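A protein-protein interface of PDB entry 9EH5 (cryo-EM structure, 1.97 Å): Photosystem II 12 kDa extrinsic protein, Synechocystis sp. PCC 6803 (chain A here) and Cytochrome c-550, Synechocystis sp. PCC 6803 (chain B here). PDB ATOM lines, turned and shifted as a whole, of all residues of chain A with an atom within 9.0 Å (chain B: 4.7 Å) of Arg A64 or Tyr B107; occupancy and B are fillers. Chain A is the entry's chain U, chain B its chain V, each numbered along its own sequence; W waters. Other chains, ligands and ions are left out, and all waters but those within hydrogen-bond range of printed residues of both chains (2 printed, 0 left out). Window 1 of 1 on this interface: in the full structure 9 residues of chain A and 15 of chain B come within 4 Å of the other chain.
OD1 of Asp A59 sits close to N of Arg A61 (3.4 Å).
The guanidinium group (NE) of Arg A64 lies within hydrogen-bond range of the backbone carbonyl oxygen (O) of Arg A61, 2.7 Å away.
NH1 of Arg A61 is in salt-bridge range of O of Tyr A131.
The backbone carbonyl oxygen (O) of Phe A69 lies within hydrogen-bond range of the backbone NH (N) of Ala A74, 3.2 Å away.
O of Tyr B107 is in hydrogen-bond range of N of Glu B88, 3.0 Å away.
OG of Ser B106 sits at hydrogen-bond distance from OD1 of Asp B108 (3.0 Å).
Asp A62 touches none of the printed residues of chain B.
Of chain B, only Asn B76, Asp B83 and Tyr B107 come within 4 Å of Arg A64.
Gly A65 touches none of the printed residues of chain B.
Printed residues of chain B within 4 Å of Gly A68: Glu B88 (3.97 Å) and Asp B108 (3.4 Å).
Of the printed residues of chain B, Phe A69 touches Asp B108.
Asp B83 touches just one residue of chain A: Arg A64 (3.6 Å).
Gly B86 touches one residue of chain A.
Of chain A, only Arg A67 (2.7 Å) comes within 4 Å of Ala B87.
Tyr B107 touches just these residues of chain A: Arg A64 and Tyr A70.
Printed residues of chain A within 4 Å of Asp B108: Gly A68 (3.4 Å), Phe A69 (3.8 Å), Tyr A70 (3.1 Å), Pro A71 (3.4 Å) and Asn A72 (2.9 Å).
The nearest printed residue of chain A that does not touch Glu B88 is Arg A102 (4.9 Å).
Water W2 bridges the side-chain amide oxygen (OD1) of Asn B76 and the backbone carbonyl oxygen (O) of Val A130.
Water W1 lies within hydrogen-bond range of O of Gly B86 (2.8 Å), O of Tyr B107 (2.9 Å), N of Gly A68 (2.9 Å) and N of Glu B88 (3.4 Å).
Among the printed residues, merely in contact across the chains: Arg A67 with Glu B88 (3.3 Å), Tyr A70 with Tyr B107 (3.4 Å), Gly A68 with Asp B108 (3.4 Å), Tyr A70 with Val B77 (3.7 Å), Phe A69 with Asp B108 (3.8 Å), Arg A64 with Tyr B107 (3.9 Å) and Gly A68 with Glu B88 (3.97 Å).
Of the 20 printed residues of chain A, 8 touch a printed residue of chain B.
Printed residues of chain A that touch a printed residue of chain B: Arg A61, Arg A64, Arg A67, Gly A68, Phe A69, Tyr A70, Pro A71 and Asn A72.
Hydrophobic or aromatic side chains of chain A that line the printed part of chain B: Tyr A70 and Pro A71.
Hydrophobic or aromatic side chains of chain B within 4 Å of the printed part of chain A: Val B77 and Tyr B107.
Along chain B the printed residues that touch a printed residue of chain A span positions 76 to 108.
Among the printed residues, Asp or Glu carboxylates within 4 Å of a Lys or Arg side-chain nitrogen of the other chain: Arg A64 with Asp B83 (3.6 Å).
NH1 of Arg A61 is in hydrogen-bond range of OD1 of Asn B76 (2.9 Å).
The guanidinium group of Arg A64 sits at hydrogen-bond distance from the backbone carbonyl oxygen of Asn B76 (3.0 Å).
The guanidinium group of Arg A64 is in salt-bridge range of the side-chain carboxylate of Asp B83 (3.6 Å).
NH1 of Arg A67 lies close to O of Gly B86.
The guanidinium group (NH1) of Arg A67 lies within hydrogen-bond range of the backbone carbonyl oxygen (O) of Ala B87 (2.7 Å).
ND2 of Asn B76 lies within hydrogen-bond range of OH of Tyr A70, at 2.7 Å.
O of Tyr A70 lies within hydrogen-bond range of N of Asp B108 (3.1 Å).
The side-chain amide oxygen (OD1) of Asn A72 sits close to the side-chain carboxylate (OD2) of Asp B108 (2.9 Å).
The backbone nitrogen (N) of Pro A71 sits close to the side-chain carboxylate (OD2) of Asp B108.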
ATOM      1  N   ILE A  53       9.772 -10.947  23.551  1.00  0.00           N
ATOM      2  CA  ILE A  53      10.321  -9.747  22.844  1.00  0.00           C
ATOM      3  C   ILE A  53      10.105  -8.466  23.645  1.00  0.00           C
ATOM      4  O   ILE A  53       8.955  -8.165  23.965  1.00  0.00           O
ATOM      5  CB  ILE A  53       9.703  -9.623  21.438  1.00  0.00           C
ATOM      6  CG1 ILE A  53       9.941 -10.877  20.599  1.00  0.00           C
ATOM      7  CG2 ILE A  53      10.198  -8.370  20.736  1.00  0.00           C
ATOM      8  CD1 ILE A  53       8.921 -11.077  19.510  1.00  0.00           C
ATOM      9  N   ASP A  59      16.456  -6.939  19.653  1.00  0.00           N
ATOM     10  CA  ASP A  59      17.054  -6.593  18.343  1.00  0.00           C
ATOM     11  C   ASP A  59      16.028  -6.884  17.255  1.00  0.00           C
ATOM     12  O   ASP A  59      15.114  -7.664  17.509  1.00  0.00           O
ATOM     13  CB  ASP A  59      18.389  -7.311  18.133  1.00  0.00           C
ATOM     14  CG  ASP A  59      18.332  -8.817  18.308  1.00  0.00           C
ATOM     15  OD1 ASP A  59      18.096  -9.511  17.305  1.00  0.00           O
ATOM     16  OD2 ASP A  59      18.543  -9.283  19.444  1.00  0.00           O
ATOM     17  N   ILE A  60      16.205  -6.306  16.082  1.00  0.00           N
ATOM     18  CA  ILE A  60      15.200  -6.435  15.031  1.00  0.00           C
ATOM     19  C   ILE A  60      14.997  -7.884  14.587  1.00  0.00           C
ATOM     20  O   ILE A  60      13.878  -8.250  14.193  1.00  0.00           O
ATOM     21  CB  ILE A  60      15.556  -5.495  13.855  1.00  0.00           C
ATOM     22  CG1 ILE A  60      14.309  -5.167  13.033  1.00  0.00           C
ATOM     23  CG2 ILE A  60      16.695  -6.031  12.981  1.00  0.00           C
ATOM     24  CD1 ILE A  60      14.410  -3.880  12.258  1.00  0.00           C
ATOM     25  N   ARG A  61      16.027  -8.735  14.723  1.00  0.00           N
ATOM     26  CA  ARG A  61      15.941 -10.130  14.298  1.00  0.00           C
ATOM     27  C   ARG A  61      14.936 -10.920  15.124  1.00  0.00           C
ATOM     28  O   ARG A  61      14.351 -11.885  14.624  1.00  0.00           O
ATOM     29  CB  ARG A  61      17.317 -10.788  14.385  1.00  0.00           C
ATOM     30  CG  ARG A  61      18.165 -10.619  13.141  1.00  0.00           C
ATOM     31  CD  ARG A  61      19.583 -11.131  13.359  1.00  0.00           C
ATOM     32  NE  ARG A  61      19.628 -12.578  13.533  1.00  0.00           N
ATOM     33  CZ  ARG A  61      19.972 -13.441  12.586  1.00  0.00           C
ATOM     34  NH1 ARG A  61      20.304 -13.040  11.370  1.00  0.00           N
ATOM     35  NH2 ARG A  61      19.986 -14.739  12.868  1.00  0.00           N
ATOM     36  N   ASP A  62      14.714 -10.521  16.378  1.00  0.00           N
ATOM     37  CA  ASP A  62      13.703 -11.161  17.210  1.00  0.00           C
ATOM     38  C   ASP A  62      12.277 -10.879  16.761  1.00  0.00           C
ATOM     39  O   ASP A  62      11.375 -11.604  17.185  1.00  0.00           O
ATOM     40  CB  ASP A  62      13.886 -10.749  18.672  1.00  0.00           C
ATOM     41  CG  ASP A  62      15.336 -10.748  19.089  1.00  0.00           C
ATOM     42  OD1 ASP A  62      16.115 -11.485  18.450  1.00  0.00           O
ATOM     43  OD2 ASP A  62      15.704 -10.021  20.036  1.00  0.00           O
ATOM     44  N   PHE A  63      12.045  -9.884  15.905  1.00  0.00           N
ATOM     45  CA  PHE A  63      10.697  -9.649  15.407  1.00  0.00           C
ATOM     46  C   PHE A  63      10.345 -10.500  14.197  1.00  0.00           C
ATOM     47  O   PHE A  63       9.222 -10.394  13.695  1.00  0.00           O
ATOM     48  CB  PHE A  63      10.508  -8.182  15.046  1.00  0.00           C
ATOM     49  CG  PHE A  63      10.404  -7.272  16.229  1.00  0.00           C
ATOM     50  CD1 PHE A  63      11.528  -6.633  16.727  1.00  0.00           C
ATOM     51  CD2 PHE A  63       9.181  -7.051  16.842  1.00  0.00           C
ATOM     52  CE1 PHE A  63      11.437  -5.794  17.821  1.00  0.00           C
ATOM     53  CE2 PHE A  63       9.081  -6.212  17.934  1.00  0.00           C
ATOM     54  CZ  PHE A  63      10.210  -5.581  18.422  1.00  0.00           C
ATOM     55  N   ARG A  64      11.271 -11.330  13.711  1.00  0.00           N
ATOM     56  CA  ARG A  64      10.985 -12.147  12.538  1.00  0.00           C
ATOM     57  C   ARG A  64      10.017 -13.279  12.858  1.00  0.00           C
ATOM     58  O   ARG A  64       9.363 -13.804  11.950  1.00  0.00           O
ATOM     59  CB  ARG A  64      12.282 -12.709  11.959  1.00  0.00           C
ATOM     60  CG  ARG A  64      13.053 -11.719  11.110  1.00  0.00           C
ATOM     61  CD  ARG A  64      14.509 -12.112  10.977  1.00  0.00           C
ATOM     62  NE  ARG A  64      15.037 -12.707  12.197  1.00  0.00           N
ATOM     63  CZ  ARG A  64      15.761 -13.816  12.238  1.00  0.00           C
ATOM     64  NH1 ARG A  64      16.043 -14.498  11.140  1.00  0.00           N
ATOM     65  NH2 ARG A  64      16.218 -14.250  13.409  1.00  0.00           N
ATOM     66  N   GLY A  65       9.904 -13.658  14.130  1.00  0.00           N
ATOM     67  CA  GLY A  65       9.003 -14.722  14.532  1.00  0.00           C
ATOM     68  C   GLY A  65       7.535 -14.363  14.471  1.00  0.00           C
ATOM     69  O   GLY A  65       6.696 -15.271  14.440  1.00  0.00           O
ATOM     70  N   LEU A  66       7.204 -13.077  14.460  1.00  0.00           N
ATOM     71  CA  LEU A  66       5.829 -12.633  14.298  1.00  0.00           C
ATOM     72  C   LEU A  66       5.592 -12.280  12.841  1.00  0.00           C
ATOM     73  O   LEU A  66       6.363 -11.518  12.247  1.00  0.00           O
ATOM     74  CB  LEU A  66       5.522 -11.435  15.191  1.00  0.00           C
ATOM     75  CG  LEU A  66       6.036 -11.535  16.620  1.00  0.00           C
ATOM     76  CD1 LEU A  66       6.048 -10.161  17.223  1.00  0.00           C
ATOM     77  CD2 LEU A  66       5.177 -12.477  17.439  1.00  0.00           C
ATOM     78  N   ARG A  67       4.523 -12.831  12.278  1.00  0.00           N
ATOM     79  CA  ARG A  67       4.271 -12.728  10.849  1.00  0.00           C
ATOM     80  C   ARG A  67       3.849 -11.309  10.498  1.00  0.00           C
ATOM     81  O   ARG A  67       2.949 -10.751  11.132  1.00  0.00           O
ATOM     82  CB  ARG A  67       3.193 -13.729  10.452  1.00  0.00           C
ATOM     83  CG  ARG A  67       2.688 -13.621   9.023  1.00  0.00           C
ATOM     84  CD  ARG A  67       1.971 -14.896   8.522  1.00  0.00           C
ATOM     85  NE  ARG A  67       2.213 -16.104   9.311  1.00  0.00           N
ATOM     86  CZ  ARG A  67       3.299 -16.864   9.219  1.00  0.00           C
ATOM     87  NH1 ARG A  67       4.251 -16.605   8.338  1.00  0.00           N
ATOM     88  NH2 ARG A  67       3.438 -17.899  10.041  1.00  0.00           N
ATOM     89  N   GLY A  68       4.506 -10.726   9.496  1.00  0.00           N
ATOM     90  CA  GLY A  68       4.220  -9.379   9.052  1.00  0.00           C
ATOM     91  C   GLY A  68       4.981  -8.274   9.756  1.00  0.00           C
ATOM     92  O   GLY A  68       4.690  -7.097   9.513  1.00  0.00           O
ATOM     93  N   PHE A  69       5.949  -8.604  10.607  1.00  0.00           N
ATOM     94  CA  PHE A  69       6.634  -7.572  11.375  1.00  0.00           C
ATOM     95  C   PHE A  69       7.935  -7.113  10.722  1.00  0.00           C
ATOM     96  O   PHE A  69       8.124  -5.915  10.494  1.00  0.00           O
ATOM     97  CB  PHE A  69       6.898  -8.072  12.795  1.00  0.00           C
ATOM     98  CG  PHE A  69       5.830  -7.686  13.771  1.00  0.00           C
ATOM     99  CD1 PHE A  69       4.582  -8.286  13.725  1.00  0.00           C
ATOM    100  CD2 PHE A  69       6.066  -6.709  14.725  1.00  0.00           C
ATOM    101  CE1 PHE A  69       3.591  -7.925  14.625  1.00  0.00           C
ATOM    102  CE2 PHE A  69       5.079  -6.345  15.621  1.00  0.00           C
ATOM    103  CZ  PHE A  69       3.842  -6.954  15.569  1.00  0.00           C
ATOM    104  N   TYR A  70       8.841  -8.036  10.446  1.00  0.00           N
ATOM    105  CA  TYR A  70      10.095  -7.690   9.789  1.00  0.00           C
ATOM    106  C   TYR A  70       9.841  -7.406   8.313  1.00  0.00           C
ATOM    107  O   TYR A  70       9.127  -8.169   7.657  1.00  0.00           O
ATOM    108  CB  TYR A  70      11.110  -8.823   9.950  1.00  0.00           C
ATOM    109  CG  TYR A  70      12.528  -8.489   9.527  1.00  0.00           C
ATOM    110  CD1 TYR A  70      12.951  -8.688   8.215  1.00  0.00           C
ATOM    111  CD2 TYR A  70      13.449  -7.992  10.442  1.00  0.00           C
ATOM    112  CE1 TYR A  70      14.241  -8.388   7.824  1.00  0.00           C
ATOM    113  CE2 TYR A  70      14.746  -7.692  10.059  1.00  0.00           C
ATOM    114  CZ  TYR A  70      15.133  -7.890   8.748  1.00  0.00           C
ATOM    115  OH  TYR A  70      16.418  -7.594   8.359  1.00  0.00           O
ATOM    116  N   PRO A  71      10.416  -6.335   7.751  1.00  0.00           N
ATOM    117  CA  PRO A  71      11.285  -5.348   8.401  1.00  0.00           C
ATOM    118  C   PRO A  71      10.605  -4.055   8.855  1.00  0.00           C
ATOM    119  O   PRO A  71      11.171  -3.337   9.664  1.00  0.00           O
ATOM    120  CB  PRO A  71      12.311  -5.060   7.304  1.00  0.00           C
ATOM    121  CG  PRO A  71      11.503  -5.127   6.039  1.00  0.00           C
ATOM    122  CD  PRO A  71      10.453  -6.196   6.282  1.00  0.00           C
ATOM    123  N   ASN A  72       9.402  -3.738   8.373  1.00  0.00           N
ATOM    124  CA  ASN A  72       8.900  -2.367   8.462  1.00  0.00           C
ATOM    125  C   ASN A  72       8.354  -2.041   9.851  1.00  0.00           C
ATOM    126  O   ASN A  72       8.752  -1.041  10.464  1.00  0.00           O
ATOM    127  CB  ASN A  72       7.832  -2.140   7.389  1.00  0.00           C
ATOM    128  CG  ASN A  72       8.397  -2.199   5.978  1.00  0.00           C
ATOM    129  OD1 ASN A  72       8.536  -3.271   5.392  1.00  0.00           O
ATOM    130  ND2 ASN A  72       8.711  -1.037   5.421  1.00  0.00           N
ATOM    131  N   ALA A  74       8.741  -3.641  12.679  1.00  0.00           N
ATOM    132  CA  ALA A  74       9.806  -3.753  13.670  1.00  0.00           C
ATOM    133  C   ALA A  74      10.693  -2.519  13.679  1.00  0.00           C
ATOM    134  O   ALA A  74      11.125  -2.063  14.746  1.00  0.00           O
ATOM    135  CB  ALA A  74      10.639  -4.992  13.382  1.00  0.00           C
ATOM    136  N   ARG A 102      -2.176  -6.032  13.455  1.00  0.00           N
ATOM    137  CA  ARG A 102      -1.067  -6.949  13.696  1.00  0.00           C
ATOM    138  C   ARG A 102      -0.461  -6.757  15.080  1.00  0.00           C
ATOM    139  O   ARG A 102      -0.092  -7.735  15.741  1.00  0.00           O
ATOM    140  CB  ARG A 102       0.000  -6.756  12.628  1.00  0.00           C
ATOM    141  CG  ARG A 102       0.729  -8.017  12.277  1.00  0.00           C
ATOM    142  CD  ARG A 102       1.611  -7.778  11.084  1.00  0.00           C
ATOM    143  NE  ARG A 102       0.852  -7.683   9.844  1.00  0.00           N
ATOM    144  CZ  ARG A 102       1.249  -6.994   8.785  1.00  0.00           C
ATOM    145  NH1 ARG A 102       2.384  -6.311   8.792  1.00  0.00           N
ATOM    146  NH2 ARG A 102       0.497  -6.994   7.690  1.00  0.00           N
ATOM    147  N   PHE A 110       4.853  -9.425  23.752  1.00  0.00           N
ATOM    148  CA  PHE A 110       5.689  -8.276  24.054  1.00  0.00           C
ATOM    149  C   PHE A 110       5.840  -8.075  25.556  1.00  0.00           C
ATOM    150  O   PHE A 110       4.925  -8.319  26.342  1.00  0.00           O
ATOM    151  CB  PHE A 110       5.109  -7.004  23.432  1.00  0.00           C
ATOM    152  CG  PHE A 110       5.002  -7.054  21.939  1.00  0.00           C
ATOM    153  CD1 PHE A 110       5.978  -7.678  21.184  1.00  0.00           C
ATOM    154  CD2 PHE A 110       3.927  -6.467  21.290  1.00  0.00           C
ATOM    155  CE1 PHE A 110       5.886  -7.716  19.813  1.00  0.00           C
ATOM    156  CE2 PHE A 110       3.829  -6.508  19.916  1.00  0.00           C
ATOM    157  CZ  PHE A 110       4.808  -7.137  19.179  1.00  0.00           C
ATOM    158  N   VAL A 130      25.413  -9.828  14.204  1.00  0.00           N
ATOM    159  CA  VAL A 130      24.922 -11.193  14.070  1.00  0.00           C
ATOM    160  C   VAL A 130      24.386 -11.367  12.656  1.00  0.00           C
ATOM    161  O   VAL A 130      23.556 -10.573  12.200  1.00  0.00           O
ATOM    162  CB  VAL A 130      23.834 -11.501  15.120  1.00  0.00           C
ATOM    163  CG1 VAL A 130      23.194 -12.852  14.860  1.00  0.00           C
ATOM    164  CG2 VAL A 130      24.420 -11.448  16.520  1.00  0.00           C
ATOM    165  N   TYR A 131      24.864 -12.395  11.964  1.00  0.00           N
ATOM    166  CA  TYR A 131      24.436 -12.652  10.596  1.00  0.00           C
ATOM    167  C   TYR A 131      24.038 -14.109  10.392  1.00  0.00           C
ATOM    168  O   TYR A 131      23.018 -14.563  10.905  1.00  0.00           O
ATOM    169  CB  TYR A 131      25.542 -12.269   9.619  1.00  0.00           C
ATOM    170  CG  TYR A 131      25.887 -10.801   9.661  1.00  0.00           C
ATOM    171  CD1 TYR A 131      25.124  -9.870   8.967  1.00  0.00           C
ATOM    172  CD2 TYR A 131      26.967 -10.345  10.404  1.00  0.00           C
ATOM    173  CE1 TYR A 131      25.431  -8.525   9.010  1.00  0.00           C
ATOM    174  CE2 TYR A 131      27.283  -9.003  10.453  1.00  0.00           C
ATOM    175  CZ  TYR A 131      26.512  -8.098   9.755  1.00  0.00           C
ATOM    176  OH  TYR A 131      26.819  -6.762   9.797  1.00  0.00           O
ATOM    177  OXT TYR A 131      24.717 -14.864   9.701  1.00  0.00           O
ATOM    178  N   ASN B  76      19.332 -12.077   7.690  1.00  0.00           N
ATOM    179  CA  ASN B  76      18.097 -12.058   8.465  1.00  0.00           C
ATOM    180  C   ASN B  76      16.972 -12.758   7.720  1.00  0.00           C
ATOM    181  O   ASN B  76      16.051 -13.290   8.345  1.00  0.00           O
ATOM    182  CB  ASN B  76      17.695 -10.620   8.790  1.00  0.00           C
ATOM    183  CG  ASN B  76      18.756  -9.885   9.573  1.00  0.00           C
ATOM    184  OD1 ASN B  76      19.668 -10.498  10.119  1.00  0.00           O
ATOM    185  ND2 ASN B  76      18.646  -8.565   9.627  1.00  0.00           N
ATOM    186  N   VAL B  77      17.032 -12.769   6.395  1.00  0.00           N
ATOM    187  CA  VAL B  77      16.011 -13.380   5.551  1.00  0.00           C
ATOM    188  C   VAL B  77      16.712 -14.487   4.769  1.00  0.00           C
ATOM    189  O   VAL B  77      17.229 -14.277   3.668  1.00  0.00           O
ATOM    190  CB  VAL B  77      15.344 -12.359   4.625  1.00  0.00           C
ATOM    191  CG1 VAL B  77      14.218 -12.986   3.849  1.00  0.00           C
ATOM    192  CG2 VAL B  77      14.816 -11.171   5.424  1.00  0.00           C
ATOM    193  N   ALA B  82      12.187 -22.234   8.916  1.00  0.00           N
ATOM    194  CA  ALA B  82      11.544 -21.315   9.849  1.00  0.00           C
ATOM    195  C   ALA B  82      11.407 -19.925   9.242  1.00  0.00           C
ATOM    196  O   ALA B  82      10.385 -19.255   9.436  1.00  0.00           O
ATOM    197  CB  ALA B  82      12.330 -21.256  11.157  1.00  0.00           C
ATOM    198  N   ASP B  83      12.420 -19.481   8.494  1.00  0.00           N
ATOM    199  CA  ASP B  83      12.348 -18.175   7.851  1.00  0.00           C
ATOM    200  C   ASP B  83      11.348 -18.178   6.701  1.00  0.00           C
ATOM    201  O   ASP B  83      10.623 -17.199   6.504  1.00  0.00           O
ATOM    202  CB  ASP B  83      13.735 -17.750   7.374  1.00  0.00           C
ATOM    203  CG  ASP B  83      14.635 -17.329   8.517  1.00  0.00           C
ATOM    204  OD1 ASP B  83      15.683 -16.702   8.262  1.00  0.00           O
ATOM    205  OD2 ASP B  83      14.293 -17.631   9.681  1.00  0.00           O
ATOM    206  N   LEU B  84      11.282 -19.274   5.941  1.00  0.00           N
ATOM    207  CA  LEU B  84      10.294 -19.363   4.871  1.00  0.00           C
ATOM    208  C   LEU B  84       8.875 -19.469   5.421  1.00  0.00           C
ATOM    209  O   LEU B  84       7.939 -18.935   4.817  1.00  0.00           O
ATOM    210  CB  LEU B  84      10.610 -20.550   3.964  1.00  0.00           C
ATOM    211  CG  LEU B  84      11.782 -20.317   3.009  1.00  0.00           C
ATOM    212  CD1 LEU B  84      12.215 -21.614   2.353  1.00  0.00           C
ATOM    213  CD2 LEU B  84      11.424 -19.279   1.962  1.00  0.00           C
ATOM    214  N   GLY B  86       7.945 -18.061   8.246  1.00  0.00           N
ATOM    215  CA  GLY B  86       7.623 -16.799   8.878  1.00  0.00           C
ATOM    216  C   GLY B  86       7.343 -15.635   7.953  1.00  0.00           C
ATOM    217  O   GLY B  86       7.016 -14.547   8.435  1.00  0.00           O
ATOM    218  N   ALA B  87       7.464 -15.822   6.642  1.00  0.00           N
ATOM    219  CA  ALA B  87       7.198 -14.743   5.700  1.00  0.00           C
ATOM    220  C   ALA B  87       5.701 -14.448   5.621  1.00  0.00           C
ATOM    221  O   ALA B  87       4.860 -15.238   6.051  1.00  0.00           O
ATOM    222  CB  ALA B  87       7.742 -15.095   4.316  1.00  0.00           C
ATOM    223  N   GLU B  88       5.377 -13.278   5.081  1.00  0.00           N
ATOM    224  CA  GLU B  88       3.987 -12.846   4.925  1.00  0.00           C
ATOM    225  C   GLU B  88       3.663 -12.672   3.446  1.00  0.00           C
ATOM    226  O   GLU B  88       4.194 -11.745   2.803  1.00  0.00           O
ATOM    227  CB  GLU B  88       3.718 -11.551   5.692  1.00  0.00           C
ATOM    228  CG  GLU B  88       2.385 -10.892   5.344  1.00  0.00           C
ATOM    229  CD  GLU B  88       1.185 -11.730   5.746  1.00  0.00           C
ATOM    230  OE1 GLU B  88       0.500 -12.258   4.845  1.00  0.00           O
ATOM    231  OE2 GLU B  88       0.905 -11.834   6.958  1.00  0.00           O
ATOM    232  N   ARG B  91       6.100 -18.802   2.845  1.00  0.00           N
ATOM    233  CA  ARG B  91       6.768 -19.178   1.607  1.00  0.00           C
ATOM    234  C   ARG B  91       7.318 -20.598   1.662  1.00  0.00           C
ATOM    235  O   ARG B  91       8.218 -20.946   0.901  1.00  0.00           O
ATOM    236  CB  ARG B  91       7.888 -18.189   1.285  1.00  0.00           C
ATOM    237  CG  ARG B  91       7.407 -16.804   0.897  1.00  0.00           C
ATOM    238  CD  ARG B  91       8.569 -15.839   0.717  1.00  0.00           C
ATOM    239  NE  ARG B  91       8.112 -14.462   0.569  1.00  0.00           N
ATOM    240  CZ  ARG B  91       8.758 -13.397   1.026  1.00  0.00           C
ATOM    241  NH1 ARG B  91       9.917 -13.507   1.654  1.00  0.00           N
ATOM    242  NH2 ARG B  91       8.228 -12.192   0.849  1.00  0.00           N
ATOM    243  N   LYS B 105       8.926  -9.611  -2.791  1.00  0.00           N
ATOM    244  CA  LYS B 105       8.503  -8.588  -1.854  1.00  0.00           C
ATOM    245  C   LYS B 105       9.455  -8.589  -0.669  1.00  0.00           C
ATOM    246  O   LYS B 105      10.390  -9.389  -0.595  1.00  0.00           O
ATOM    247  CB  LYS B 105       7.064  -8.818  -1.379  1.00  0.00           C
ATOM    248  CG  LYS B 105       6.056  -9.036  -2.489  1.00  0.00           C
ATOM    249  CD  LYS B 105       5.457  -7.719  -2.953  1.00  0.00           C
ATOM    250  CE  LYS B 105       4.150  -7.934  -3.696  1.00  0.00           C
ATOM    251  NZ  LYS B 105       3.969  -9.340  -4.147  1.00  0.00           N
ATOM    252  N   SER B 106       9.198  -7.689   0.275  1.00  0.00           N
ATOM    253  CA  SER B 106       9.866  -7.749   1.560  1.00  0.00           C
ATOM    254  C   SER B 106       9.291  -8.904   2.379  1.00  0.00           C
ATOM    255  O   SER B 106       8.318  -9.556   1.989  1.00  0.00           O
ATOM    256  CB  SER B 106       9.728  -6.419   2.299  1.00  0.00           C
ATOM    257  OG  SER B 106       8.481  -5.809   2.020  1.00  0.00           O
ATOM    258  N   TYR B 107       9.912  -9.154   3.534  1.00  0.00           N
ATOM    259  CA  TYR B 107       9.537 -10.274   4.388  1.00  0.00           C
ATOM    260  C   TYR B 107       8.120 -10.156   4.941  1.00  0.00           C
ATOM    261  O   TYR B 107       7.490 -11.184   5.209  1.00  0.00           O
ATOM    262  CB  TYR B 107      10.536 -10.390   5.534  1.00  0.00           C
ATOM    263  CG  TYR B 107      10.517 -11.720   6.228  1.00  0.00           C
ATOM    264  CD1 TYR B 107      10.863 -12.877   5.550  1.00  0.00           C
ATOM    265  CD2 TYR B 107      10.160 -11.819   7.566  1.00  0.00           C
ATOM    266  CE1 TYR B 107      10.853 -14.092   6.177  1.00  0.00           C
ATOM    267  CE2 TYR B 107      10.143 -13.039   8.207  1.00  0.00           C
ATOM    268  CZ  TYR B 107      10.491 -14.171   7.506  1.00  0.00           C
ATOM    269  OH  TYR B 107      10.487 -15.387   8.139  1.00  0.00           O
ATOM    270  N   ASP B 108       7.607  -8.938   5.104  1.00  0.00           N
ATOM    271  CA  ASP B 108       6.218  -8.717   5.482  1.00  0.00           C
ATOM    272  C   ASP B 108       5.307  -8.530   4.279  1.00  0.00           C
ATOM    273  O   ASP B 108       4.124  -8.222   4.456  1.00  0.00           O
ATOM    274  CB  ASP B 108       6.099  -7.503   6.410  1.00  0.00           C
ATOM    275  CG  ASP B 108       6.946  -6.325   5.959  1.00  0.00           C
ATOM    276  OD1 ASP B 108       7.361  -6.275   4.785  1.00  0.00           O
ATOM    277  OD2 ASP B 108       7.203  -5.439   6.797  1.00  0.00           O
ATOM    278  N   GLY B 109       5.837  -8.690   3.069  1.00  0.00           N
ATOM    279  CA  GLY B 109       5.069  -8.532   1.852  1.00  0.00           C
ATOM    280  C   GLY B 109       4.576  -7.131   1.577  1.00  0.00           C
ATOM    281  O   GLY B 109       3.503  -6.969   0.994  1.00  0.00           O
HETATM  282  O   HOH W   1       6.619 -11.850   7.872  1.00  0.00           O
HETATM  283  O   HOH W   2      21.951  -9.736  10.040  1.00  0.00           O
